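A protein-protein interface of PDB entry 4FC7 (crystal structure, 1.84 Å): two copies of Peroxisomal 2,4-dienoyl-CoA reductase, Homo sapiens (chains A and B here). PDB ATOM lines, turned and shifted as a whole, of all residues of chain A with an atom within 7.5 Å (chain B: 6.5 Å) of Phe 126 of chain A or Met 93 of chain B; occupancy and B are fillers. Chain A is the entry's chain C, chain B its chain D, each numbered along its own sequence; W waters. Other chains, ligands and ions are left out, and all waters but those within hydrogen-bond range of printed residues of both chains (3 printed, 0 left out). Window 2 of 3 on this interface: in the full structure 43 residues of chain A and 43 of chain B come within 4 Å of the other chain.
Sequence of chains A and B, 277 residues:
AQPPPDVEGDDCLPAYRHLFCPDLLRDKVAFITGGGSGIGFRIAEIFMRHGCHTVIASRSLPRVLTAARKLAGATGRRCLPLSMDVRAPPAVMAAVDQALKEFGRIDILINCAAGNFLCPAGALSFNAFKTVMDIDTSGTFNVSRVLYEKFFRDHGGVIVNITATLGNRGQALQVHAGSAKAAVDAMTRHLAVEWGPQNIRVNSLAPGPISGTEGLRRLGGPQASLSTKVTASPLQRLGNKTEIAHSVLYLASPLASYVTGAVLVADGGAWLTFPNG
O of Ser 138 of chain B sits close to OD1 of Asn 142 of chain B, 3.3 Å away.
The side-chain hydroxyl (OG) of Ser 125 of chain A lies within hydrogen-bond range of the backbone NH (N) of Ala 128 of chain A (2.9 Å).
Met 93 of chain B touches just one residue of chain A: Phe 126 (3.3 Å).
Of the printed residues of chain A, Arg 145 of chain B touches Ala 123 (3.8 Å), Leu 124 (2.9 Å) and Phe 126 (3.6 Å).
Printed residues of chain A within 4 Å of Pro 89 of chain B: Phe 126 (3.5 Å).
Of the printed residues of chain B, Ala 123 of chain A touches Arg 145 (3.8 Å).
Of the printed residues of chain A, Phe 141 of chain B touches Leu 124 (3.5 Å), Ser 125 (3.9 Å) and Phe 129 (3.7 Å).
Printed residues of chain A within 4 Å of Val 146 of chain B: Phe 126.
Gln 98 of chain B touches none of the printed residues of chain A.
The nearest printed residue of chain A that does not touch Met 93 of chain B is Ser 125 of chain A (8.5 Å).
The nearest printed residue of chain B that does not touch Ala 123 of chain A is Phe 141 of chain B (6.3 Å).
Ala 123 of chain A touches Arg 145 of chain B (C to NH2, 3.8 Å).
Phe 141 of chain B touches Leu 124 of chain A.
Ser 125 of chain A touches Phe 141 of chain B.
Pro 89 of chain B touches Phe 126 of chain A.
CE2 of Phe 126 of chain A touches CE of Met 93 of chain B, at 3.3 Å.
OD1 of Asn 142 of chain B touches CD1 of Phe 126 of chain A, at 3.0 Å.
Val 146 of chain B touches Phe 126 of chain A (CG2 to CZ, 3.7 Å).
Phe 129 of chain A touches Ser 138 of chain B.
CB of Phe 129 of chain A touches CD2 of Phe 141 of chain B, at 3.7 Å.
CG of Lys 130 of chain A touches OG of Ser 138 of chain B, 3.8 Å away.
No position is printed for both chains.
Of the 12 pairs that touch across the chains among the printed residues, none has its exchanged pair printed and touching as well.
The backbone carbonyl oxygen of Leu 124 of chain A sits at hydrogen-bond distance from the guanidinium group of Arg 145 of chain B, at 2.9 Å.
Printed residues of chain A that touch a printed residue of chain B: Ala 123, Leu 124, Ser 125, Phe 126, Phe 129 and Lys 130.
Among the printed residues, 12 pairs touch across the chains.
Among the printed residues, no Asp or Glu carboxylate lies within 4 Å of a Lys or Arg side-chain nitrogen of the other chain.
Water W3 bridges NE of Arg 145 of chain B (2.6 Å) and O of Leu 124 of chain A (3.0 Å).
Water W2 bridges O of Phe 126 of chain A (2.7 Å) and OD1 of Asn 142 of chain B (2.8 Å).
Water W1 bridges O of Ala 123 of chain A (3.2 Å) and NH2 of Arg 145 of chain B (3.3 Å).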
ATOM      1  N   ALA A 123      -3.315  -6.158  -6.494  1.00  0.00           N
ATOM      2  CA  ALA A 123      -4.784  -5.860  -6.583  1.00  0.00           C
ATOM      3  C   ALA A 123      -5.232  -4.854  -5.540  1.00  0.00           C
ATOM      4  O   ALA A 123      -6.356  -4.417  -5.579  1.00  0.00           O
ATOM      5  CB  ALA A 123      -5.659  -7.140  -6.406  1.00  0.00           C
ATOM      6  N   LEU A 124      -4.392  -4.601  -4.526  1.00  0.00           N
ATOM      7  CA  LEU A 124      -4.752  -3.736  -3.373  1.00  0.00           C
ATOM      8  C   LEU A 124      -4.866  -2.286  -3.801  1.00  0.00           C
ATOM      9  O   LEU A 124      -3.900  -1.723  -4.378  1.00  0.00           O
ATOM     10  CB  LEU A 124      -3.678  -3.848  -2.277  1.00  0.00           C
ATOM     11  CG  LEU A 124      -4.126  -3.222  -0.982  1.00  0.00           C
ATOM     12  CD1 LEU A 124      -5.303  -4.028  -0.401  1.00  0.00           C
ATOM     13  CD2 LEU A 124      -2.886  -3.278  -0.016  1.00  0.00           C
ATOM     14  N   SER A 125      -6.041  -1.690  -3.614  1.00  0.00           N
ATOM     15  CA  SER A 125      -6.145  -0.292  -4.027  1.00  0.00           C
ATOM     16  C   SER A 125      -5.375   0.636  -3.033  1.00  0.00           C
ATOM     17  O   SER A 125      -5.033   0.253  -1.892  1.00  0.00           O
ATOM     18  CB  SER A 125      -7.625   0.122  -4.078  1.00  0.00           C
ATOM     19  OG  SER A 125      -8.136   0.326  -2.735  1.00  0.00           O
ATOM     20  N   PHE A 126      -5.122   1.860  -3.463  1.00  0.00           N
ATOM     21  CA  PHE A 126      -4.423   2.828  -2.688  1.00  0.00           C
ATOM     22  C   PHE A 126      -5.227   3.134  -1.406  1.00  0.00           C
ATOM     23  O   PHE A 126      -4.649   3.239  -0.355  1.00  0.00           O
ATOM     24  CB  PHE A 126      -4.322   4.102  -3.504  1.00  0.00           C
ATOM     25  CG  PHE A 126      -3.807   3.856  -4.885  1.00  0.00           C
ATOM     26  CD1 PHE A 126      -2.459   3.545  -5.079  1.00  0.00           C
ATOM     27  CD2 PHE A 126      -4.699   3.889  -6.009  1.00  0.00           C
ATOM     28  CE1 PHE A 126      -1.971   3.289  -6.355  1.00  0.00           C
ATOM     29  CE2 PHE A 126      -4.199   3.635  -7.296  1.00  0.00           C
ATOM     30  CZ  PHE A 126      -2.837   3.342  -7.449  1.00  0.00           C
ATOM     31  N   ASN A 127      -6.534   3.337  -1.568  1.00  0.00           N
ATOM     32  CA  ASN A 127      -7.431   3.528  -0.439  1.00  0.00           C
ATOM     33  C   ASN A 127      -7.522   2.313   0.528  1.00  0.00           C
ATOM     34  O   ASN A 127      -7.688   2.476   1.754  1.00  0.00           O
ATOM     35  CB  ASN A 127      -8.841   3.881  -0.904  1.00  0.00           C
ATOM     36  CG  ASN A 127      -9.729   4.292   0.256  1.00  0.00           C
ATOM     37  OD1 ASN A 127      -9.322   5.119   1.102  1.00  0.00           O
ATOM     38  ND2 ASN A 127     -10.945   3.743   0.303  1.00  0.00           N
ATOM     39  N   ALA A 128      -7.453   1.109  -0.001  1.00  0.00           N
ATOM     40  CA  ALA A 128      -7.504  -0.053   0.868  1.00  0.00           C
ATOM     41  C   ALA A 128      -6.225  -0.091   1.777  1.00  0.00           C
ATOM     42  O   ALA A 128      -6.316  -0.282   2.998  1.00  0.00           O
ATOM     43  CB  ALA A 128      -7.684  -1.320   0.045  1.00  0.00           C
ATOM     44  N   PHE A 129      -5.065   0.160   1.167  1.00  0.00           N
ATOM     45  CA  PHE A 129      -3.820   0.169   1.931  1.00  0.00           C
ATOM     46  C   PHE A 129      -3.873   1.218   3.007  1.00  0.00           C
ATOM     47  O   PHE A 129      -3.574   0.927   4.197  1.00  0.00           O
ATOM     48  CB  PHE A 129      -2.596   0.405   1.006  1.00  0.00           C
ATOM     49  CG  PHE A 129      -1.280   0.407   1.724  1.00  0.00           C
ATOM     50  CD1 PHE A 129      -0.581  -0.797   1.923  1.00  0.00           C
ATOM     51  CD2 PHE A 129      -0.748   1.585   2.260  1.00  0.00           C
ATOM     52  CE1 PHE A 129       0.636  -0.852   2.627  1.00  0.00           C
ATOM     53  CE2 PHE A 129       0.481   1.526   2.912  1.00  0.00           C
ATOM     54  CZ  PHE A 129       1.147   0.335   3.130  1.00  0.00           C
ATOM     55  N   LYS A 130      -4.236   2.436   2.614  1.00  0.00           N
ATOM     56  CA  LYS A 130      -4.300   3.564   3.516  1.00  0.00           C
ATOM     57  C   LYS A 130      -5.276   3.351   4.706  1.00  0.00           C
ATOM     58  O   LYS A 130      -4.999   3.795   5.847  1.00  0.00           O
ATOM     59  CB  LYS A 130      -4.735   4.830   2.748  1.00  0.00           C
ATOM     60  CG  LYS A 130      -4.473   6.095   3.521  1.00  0.00           C
ATOM     61  CD  LYS A 130      -4.488   7.326   2.615  1.00  0.00           C
ATOM     62  CE  LYS A 130      -5.110   8.550   3.314  1.00  0.00           C
ATOM     63  NZ  LYS A 130      -4.680   8.918   4.720  1.00  0.00           N
ATOM     64  N   THR A 131      -6.406   2.713   4.411  1.00  0.00           N
ATOM     65  CA  THR A 131      -7.471   2.439   5.375  1.00  0.00           C
ATOM     66  C   THR A 131      -6.914   1.520   6.477  1.00  0.00           C
ATOM     67  O   THR A 131      -7.164   1.763   7.660  1.00  0.00           O
ATOM     68  CB  THR A 131      -8.694   1.813   4.725  1.00  0.00           C
ATOM     69  OG1 THR A 131      -9.206   2.741   3.783  1.00  0.00           O
ATOM     70  CG2 THR A 131      -9.818   1.420   5.768  1.00  0.00           C
ATOM     71  N   VAL A 132      -6.170   0.475   6.095  1.00  0.00           N
ATOM     72  CA  VAL A 132      -5.559  -0.363   7.097  1.00  0.00           C
ATOM     73  C   VAL A 132      -4.477   0.410   7.861  1.00  0.00           C
ATOM     74  O   VAL A 132      -4.434   0.320   9.137  1.00  0.00           O
ATOM     75  CB  VAL A 132      -5.034  -1.676   6.495  1.00  0.00           C
ATOM     76  CG1 VAL A 132      -4.208  -2.463   7.537  1.00  0.00           C
ATOM     77  CG2 VAL A 132      -6.240  -2.479   6.039  1.00  0.00           C
ATOM     78  N   MET B  84       4.591  15.728  -8.775  1.00  0.00           N
ATOM     79  CA  MET B  84       3.567  14.847  -8.309  1.00  0.00           C
ATOM     80  C   MET B  84       3.727  14.666  -6.816  1.00  0.00           C
ATOM     81  O   MET B  84       4.840  14.484  -6.331  1.00  0.00           O
ATOM     82  CB  MET B  84       3.581  13.433  -8.967  1.00  0.00           C
ATOM     83  CG  MET B  84       4.894  12.727  -9.014  1.00  0.00           C
ATOM     84  SD  MET B  84       4.918  10.877  -8.937  1.00  0.00           S
ATOM     85  CE  MET B  84       5.683  10.725  -7.306  1.00  0.00           C
ATOM     86  N   ALA B  88      -1.186  11.307  -3.907  1.00  0.00           N
ATOM     87  CA  ALA B  88      -2.313  11.535  -4.876  1.00  0.00           C
ATOM     88  C   ALA B  88      -2.129  10.512  -6.029  1.00  0.00           C
ATOM     89  O   ALA B  88      -1.321  10.755  -6.966  1.00  0.00           O
ATOM     90  CB  ALA B  88      -2.265  12.975  -5.387  1.00  0.00           C
ATOM     91  N   PRO B  89      -2.804   9.330  -5.943  1.00  0.00           N
ATOM     92  CA  PRO B  89      -2.607   8.342  -7.009  1.00  0.00           C
ATOM     93  C   PRO B  89      -2.882   8.821  -8.468  1.00  0.00           C
ATOM     94  O   PRO B  89      -2.108   8.418  -9.300  1.00  0.00           O
ATOM     95  CB  PRO B  89      -3.483   7.140  -6.612  1.00  0.00           C
ATOM     96  CG  PRO B  89      -3.798   7.357  -5.146  1.00  0.00           C
ATOM     97  CD  PRO B  89      -3.754   8.855  -4.909  1.00  0.00           C
ATOM     98  N   PRO B  90      -3.847   9.764  -8.729  1.00  0.00           N
ATOM     99  CA  PRO B  90      -3.963  10.328 -10.126  1.00  0.00           C
ATOM    100  C   PRO B  90      -2.685  10.995 -10.621  1.00  0.00           C
ATOM    101  O   PRO B  90      -2.319  10.849 -11.805  1.00  0.00           O
ATOM    102  CB  PRO B  90      -5.053  11.381  -9.992  1.00  0.00           C
ATOM    103  CG  PRO B  90      -5.945  10.777  -8.953  1.00  0.00           C
ATOM    104  CD  PRO B  90      -5.016  10.180  -7.918  1.00  0.00           C
ATOM    105  N   ALA B  91      -2.032  11.722  -9.718  1.00  0.00           N
ATOM    106  CA  ALA B  91      -0.802  12.422 -10.121  1.00  0.00           C
ATOM    107  C   ALA B  91       0.343  11.448 -10.346  1.00  0.00           C
ATOM    108  O   ALA B  91       1.159  11.646 -11.229  1.00  0.00           O
ATOM    109  CB  ALA B  91      -0.436  13.412  -9.075  1.00  0.00           C
ATOM    110  N   VAL B  92       0.409  10.412  -9.528  1.00  0.00           N
ATOM    111  CA  VAL B  92       1.464   9.452  -9.642  1.00  0.00           C
ATOM    112  C   VAL B  92       1.262   8.726 -11.004  1.00  0.00           C
ATOM    113  O   VAL B  92       2.237   8.479 -11.733  1.00  0.00           O
ATOM    114  CB  VAL B  92       1.423   8.467  -8.484  1.00  0.00           C
ATOM    115  CG1 VAL B  92       2.433   7.362  -8.722  1.00  0.00           C
ATOM    116  CG2 VAL B  92       1.767   9.222  -7.152  1.00  0.00           C
ATOM    117  N   MET B  93       0.013   8.399 -11.306  1.00  0.00           N
ATOM    118  CA  MET B  93      -0.309   7.676 -12.587  1.00  0.00           C
ATOM    119  C   MET B  93       0.086   8.559 -13.793  1.00  0.00           C
ATOM    120  O   MET B  93       0.664   8.088 -14.761  1.00  0.00           O
ATOM    121  CB  MET B  93      -1.784   7.345 -12.678  1.00  0.00           C
ATOM    122  CG  MET B  93      -2.119   6.088 -11.911  1.00  0.00           C
ATOM    123  SD  MET B  93      -3.890   5.685 -11.824  1.00  0.00           S
ATOM    124  CE  MET B  93      -4.148   5.400 -10.079  1.00  0.00           C
ATOM    125  N   ALA B  94      -0.149   9.874 -13.651  1.00  0.00           N
ATOM    126  CA  ALA B  94       0.147  10.801 -14.722  1.00  0.00           C
ATOM    127  C   ALA B  94       1.668  10.931 -14.941  1.00  0.00           C
ATOM    128  O   ALA B  94       2.128  11.003 -16.082  1.00  0.00           O
ATOM    129  CB  ALA B  94      -0.490  12.127 -14.405  1.00  0.00           C
ATOM    130  N   ALA B  95       2.450  10.973 -13.854  1.00  0.00           N
ATOM    131  CA  ALA B  95       3.902  11.133 -13.955  1.00  0.00           C
ATOM    132  C   ALA B  95       4.496   9.867 -14.575  1.00  0.00           C
ATOM    133  O   ALA B  95       5.469   9.888 -15.377  1.00  0.00           O
ATOM    134  CB  ALA B  95       4.468  11.310 -12.534  1.00  0.00           C
ATOM    135  N   VAL B  96       3.963   8.720 -14.165  1.00  0.00           N
ATOM    136  CA  VAL B  96       4.492   7.462 -14.652  1.00  0.00           C
ATOM    137  C   VAL B  96       4.144   7.371 -16.159  1.00  0.00           C
ATOM    138  O   VAL B  96       5.011   6.976 -16.953  1.00  0.00           O
ATOM    139  CB  VAL B  96       3.992   6.265 -13.859  1.00  0.00           C
ATOM    140  CG1 VAL B  96       4.429   4.981 -14.586  1.00  0.00           C
ATOM    141  CG2 VAL B  96       4.611   6.338 -12.439  1.00  0.00           C
ATOM    142  N   ASP B  97       2.915   7.752 -16.534  1.00  0.00           N
ATOM    143  CA  ASP B  97       2.563   7.813 -17.967  1.00  0.00           C
ATOM    144  C   ASP B  97       3.473   8.752 -18.772  1.00  0.00           C
ATOM    145  O   ASP B  97       3.841   8.413 -19.888  1.00  0.00           O
ATOM    146  CB  ASP B  97       1.138   8.317 -18.193  1.00  0.00           C
ATOM    147  CG  ASP B  97       0.083   7.336 -17.724  1.00  0.00           C
ATOM    148  OD1 ASP B  97       0.169   6.126 -18.042  1.00  0.00           O
ATOM    149  OD2 ASP B  97      -0.879   7.795 -17.054  1.00  0.00           O
ATOM    150  N   GLN B  98       3.815   9.919 -18.217  1.00  0.00           N
ATOM    151  CA  GLN B  98       4.746  10.797 -18.874  1.00  0.00           C
ATOM    152  C   GLN B  98       6.174  10.232 -19.058  1.00  0.00           C
ATOM    153  O   GLN B  98       6.737  10.361 -20.138  1.00  0.00           O
ATOM    154  CB  GLN B  98       4.806  12.161 -18.241  1.00  0.00           C
ATOM    155  CG  GLN B  98       3.521  12.924 -18.377  1.00  0.00           C
ATOM    156  CD  GLN B  98       3.323  13.369 -19.797  1.00  0.00           C
ATOM    157  OE1 GLN B  98       2.271  13.107 -20.408  1.00  0.00           O
ATOM    158  NE2 GLN B  98       4.346  14.000 -20.359  1.00  0.00           N
ATOM    159  N   SER B 138       2.152   5.126   2.795  1.00  0.00           N
ATOM    160  CA  SER B 138       1.211   5.162   1.739  1.00  0.00           C
ATOM    161  C   SER B 138       1.817   5.672   0.420  1.00  0.00           C
ATOM    162  O   SER B 138       1.554   5.051  -0.603  1.00  0.00           O
ATOM    163  CB  SER B 138      -0.086   5.932   2.110  1.00  0.00           C
ATOM    164  OG  SER B 138      -0.793   5.147   3.068  1.00  0.00           O
ATOM    165  N   PHE B 141       3.968   2.835  -1.102  1.00  0.00           N
ATOM    166  CA  PHE B 141       3.056   1.803  -1.653  1.00  0.00           C
ATOM    167  C   PHE B 141       2.461   2.302  -2.986  1.00  0.00           C
ATOM    168  O   PHE B 141       2.448   1.580  -3.959  1.00  0.00           O
ATOM    169  CB  PHE B 141       1.919   1.376  -0.722  1.00  0.00           C
ATOM    170  CG  PHE B 141       0.931   0.451  -1.385  1.00  0.00           C
ATOM    171  CD1 PHE B 141       1.286  -0.866  -1.635  1.00  0.00           C
ATOM    172  CD2 PHE B 141      -0.262   0.929  -1.837  1.00  0.00           C
ATOM    173  CE1 PHE B 141       0.375  -1.774  -2.241  1.00  0.00           C
ATOM    174  CE2 PHE B 141      -1.175   0.086  -2.436  1.00  0.00           C
ATOM    175  CZ  PHE B 141      -0.872  -1.264  -2.655  1.00  0.00           C
ATOM    176  N   ASN B 142       1.975   3.550  -2.968  1.00  0.00           N
ATOM    177  CA  ASN B 142       1.268   4.085  -4.165  1.00  0.00           C
ATOM    178  C   ASN B 142       2.196   4.072  -5.362  1.00  0.00           C
ATOM    179  O   ASN B 142       1.741   3.665  -6.431  1.00  0.00           O
ATOM    180  CB  ASN B 142       0.736   5.532  -3.999  1.00  0.00           C
ATOM    181  CG  ASN B 142      -0.414   5.630  -2.981  1.00  0.00           C
ATOM    182  OD1 ASN B 142      -1.058   4.647  -2.659  1.00  0.00           O
ATOM    183  ND2 ASN B 142      -0.669   6.866  -2.463  1.00  0.00           N
ATOM    184  N   VAL B 143       3.412   4.630  -5.220  1.00  0.00           N
ATOM    185  CA  VAL B 143       4.285   4.681  -6.372  1.00  0.00           C
ATOM    186  C   VAL B 143       4.652   3.266  -6.852  1.00  0.00           C
ATOM    187  O   VAL B 143       4.717   3.001  -8.058  1.00  0.00           O
ATOM    188  CB  VAL B 143       5.534   5.539  -6.136  1.00  0.00           C
ATOM    189  CG1 VAL B 143       6.373   5.614  -7.443  1.00  0.00           C
ATOM    190  CG2 VAL B 143       5.104   6.966  -5.633  1.00  0.00           C
ATOM    191  N   ARG B 145       3.019   0.476  -6.516  1.00  0.00           N
ATOM    192  CA  ARG B 145       1.874  -0.218  -7.068  1.00  0.00           C
ATOM    193  C   ARG B 145       1.524   0.348  -8.465  1.00  0.00           C
ATOM    194  O   ARG B 145       1.138  -0.450  -9.349  1.00  0.00           O
ATOM    195  CB  ARG B 145       0.687  -0.031  -6.080  1.00  0.00           C
ATOM    196  CG  ARG B 145      -0.739  -0.064  -6.491  1.00  0.00           C
ATOM    197  CD  ARG B 145      -1.059  -1.571  -6.520  1.00  0.00           C
ATOM    198  NE  ARG B 145      -2.454  -1.923  -6.872  1.00  0.00           N
ATOM    199  CZ  ARG B 145      -2.971  -1.965  -8.103  1.00  0.00           C
ATOM    200  NH1 ARG B 145      -2.255  -1.629  -9.186  1.00  0.00           N
ATOM    201  NH2 ARG B 145      -4.245  -2.341  -8.259  1.00  0.00           N
ATOM    202  N   VAL B 146       1.600   1.672  -8.643  1.00  0.00           N
ATOM    203  CA  VAL B 146       1.473   2.266  -9.983  1.00  0.00           C
ATOM    204  C   VAL B 146       2.549   1.698 -10.959  1.00  0.00           C
ATOM    205  O   VAL B 146       2.226   1.224 -12.034  1.00  0.00           O
ATOM    206  CB  VAL B 146       1.531   3.814  -9.933  1.00  0.00           C
ATOM    207  CG1 VAL B 146       1.457   4.353 -11.400  1.00  0.00           C
ATOM    208  CG2 VAL B 146       0.321   4.378  -9.113  1.00  0.00           C
ATOM    209  N   LYS B 150       1.781  -0.357 -14.348  1.00  0.00           N
ATOM    210  CA  LYS B 150       2.114   0.331 -15.624  1.00  0.00           C
ATOM    211  C   LYS B 150       3.282  -0.288 -16.361  1.00  0.00           C
ATOM    212  O   LYS B 150       3.450  -0.049 -17.565  1.00  0.00           O
ATOM    213  CB  LYS B 150       2.365   1.834 -15.388  1.00  0.00           C
ATOM    214  CG  LYS B 150       1.051   2.475 -14.980  1.00  0.00           C
ATOM    215  CD  LYS B 150       0.975   3.834 -15.562  1.00  0.00           C
ATOM    216  CE  LYS B 150      -0.260   4.539 -15.057  1.00  0.00           C
ATOM    217  NZ  LYS B 150      -1.167   4.694 -16.222  1.00  0.00           N
HETATM  218  O   HOH W   1      -7.183  -1.718  -7.017  1.00  0.00           O
HETATM  219  O   HOH W   2      -2.177   4.227  -0.099  1.00  0.00           O
HETATM  220  O   HOH W   3      -3.583   0.416  -6.491  1.00  0.00           O
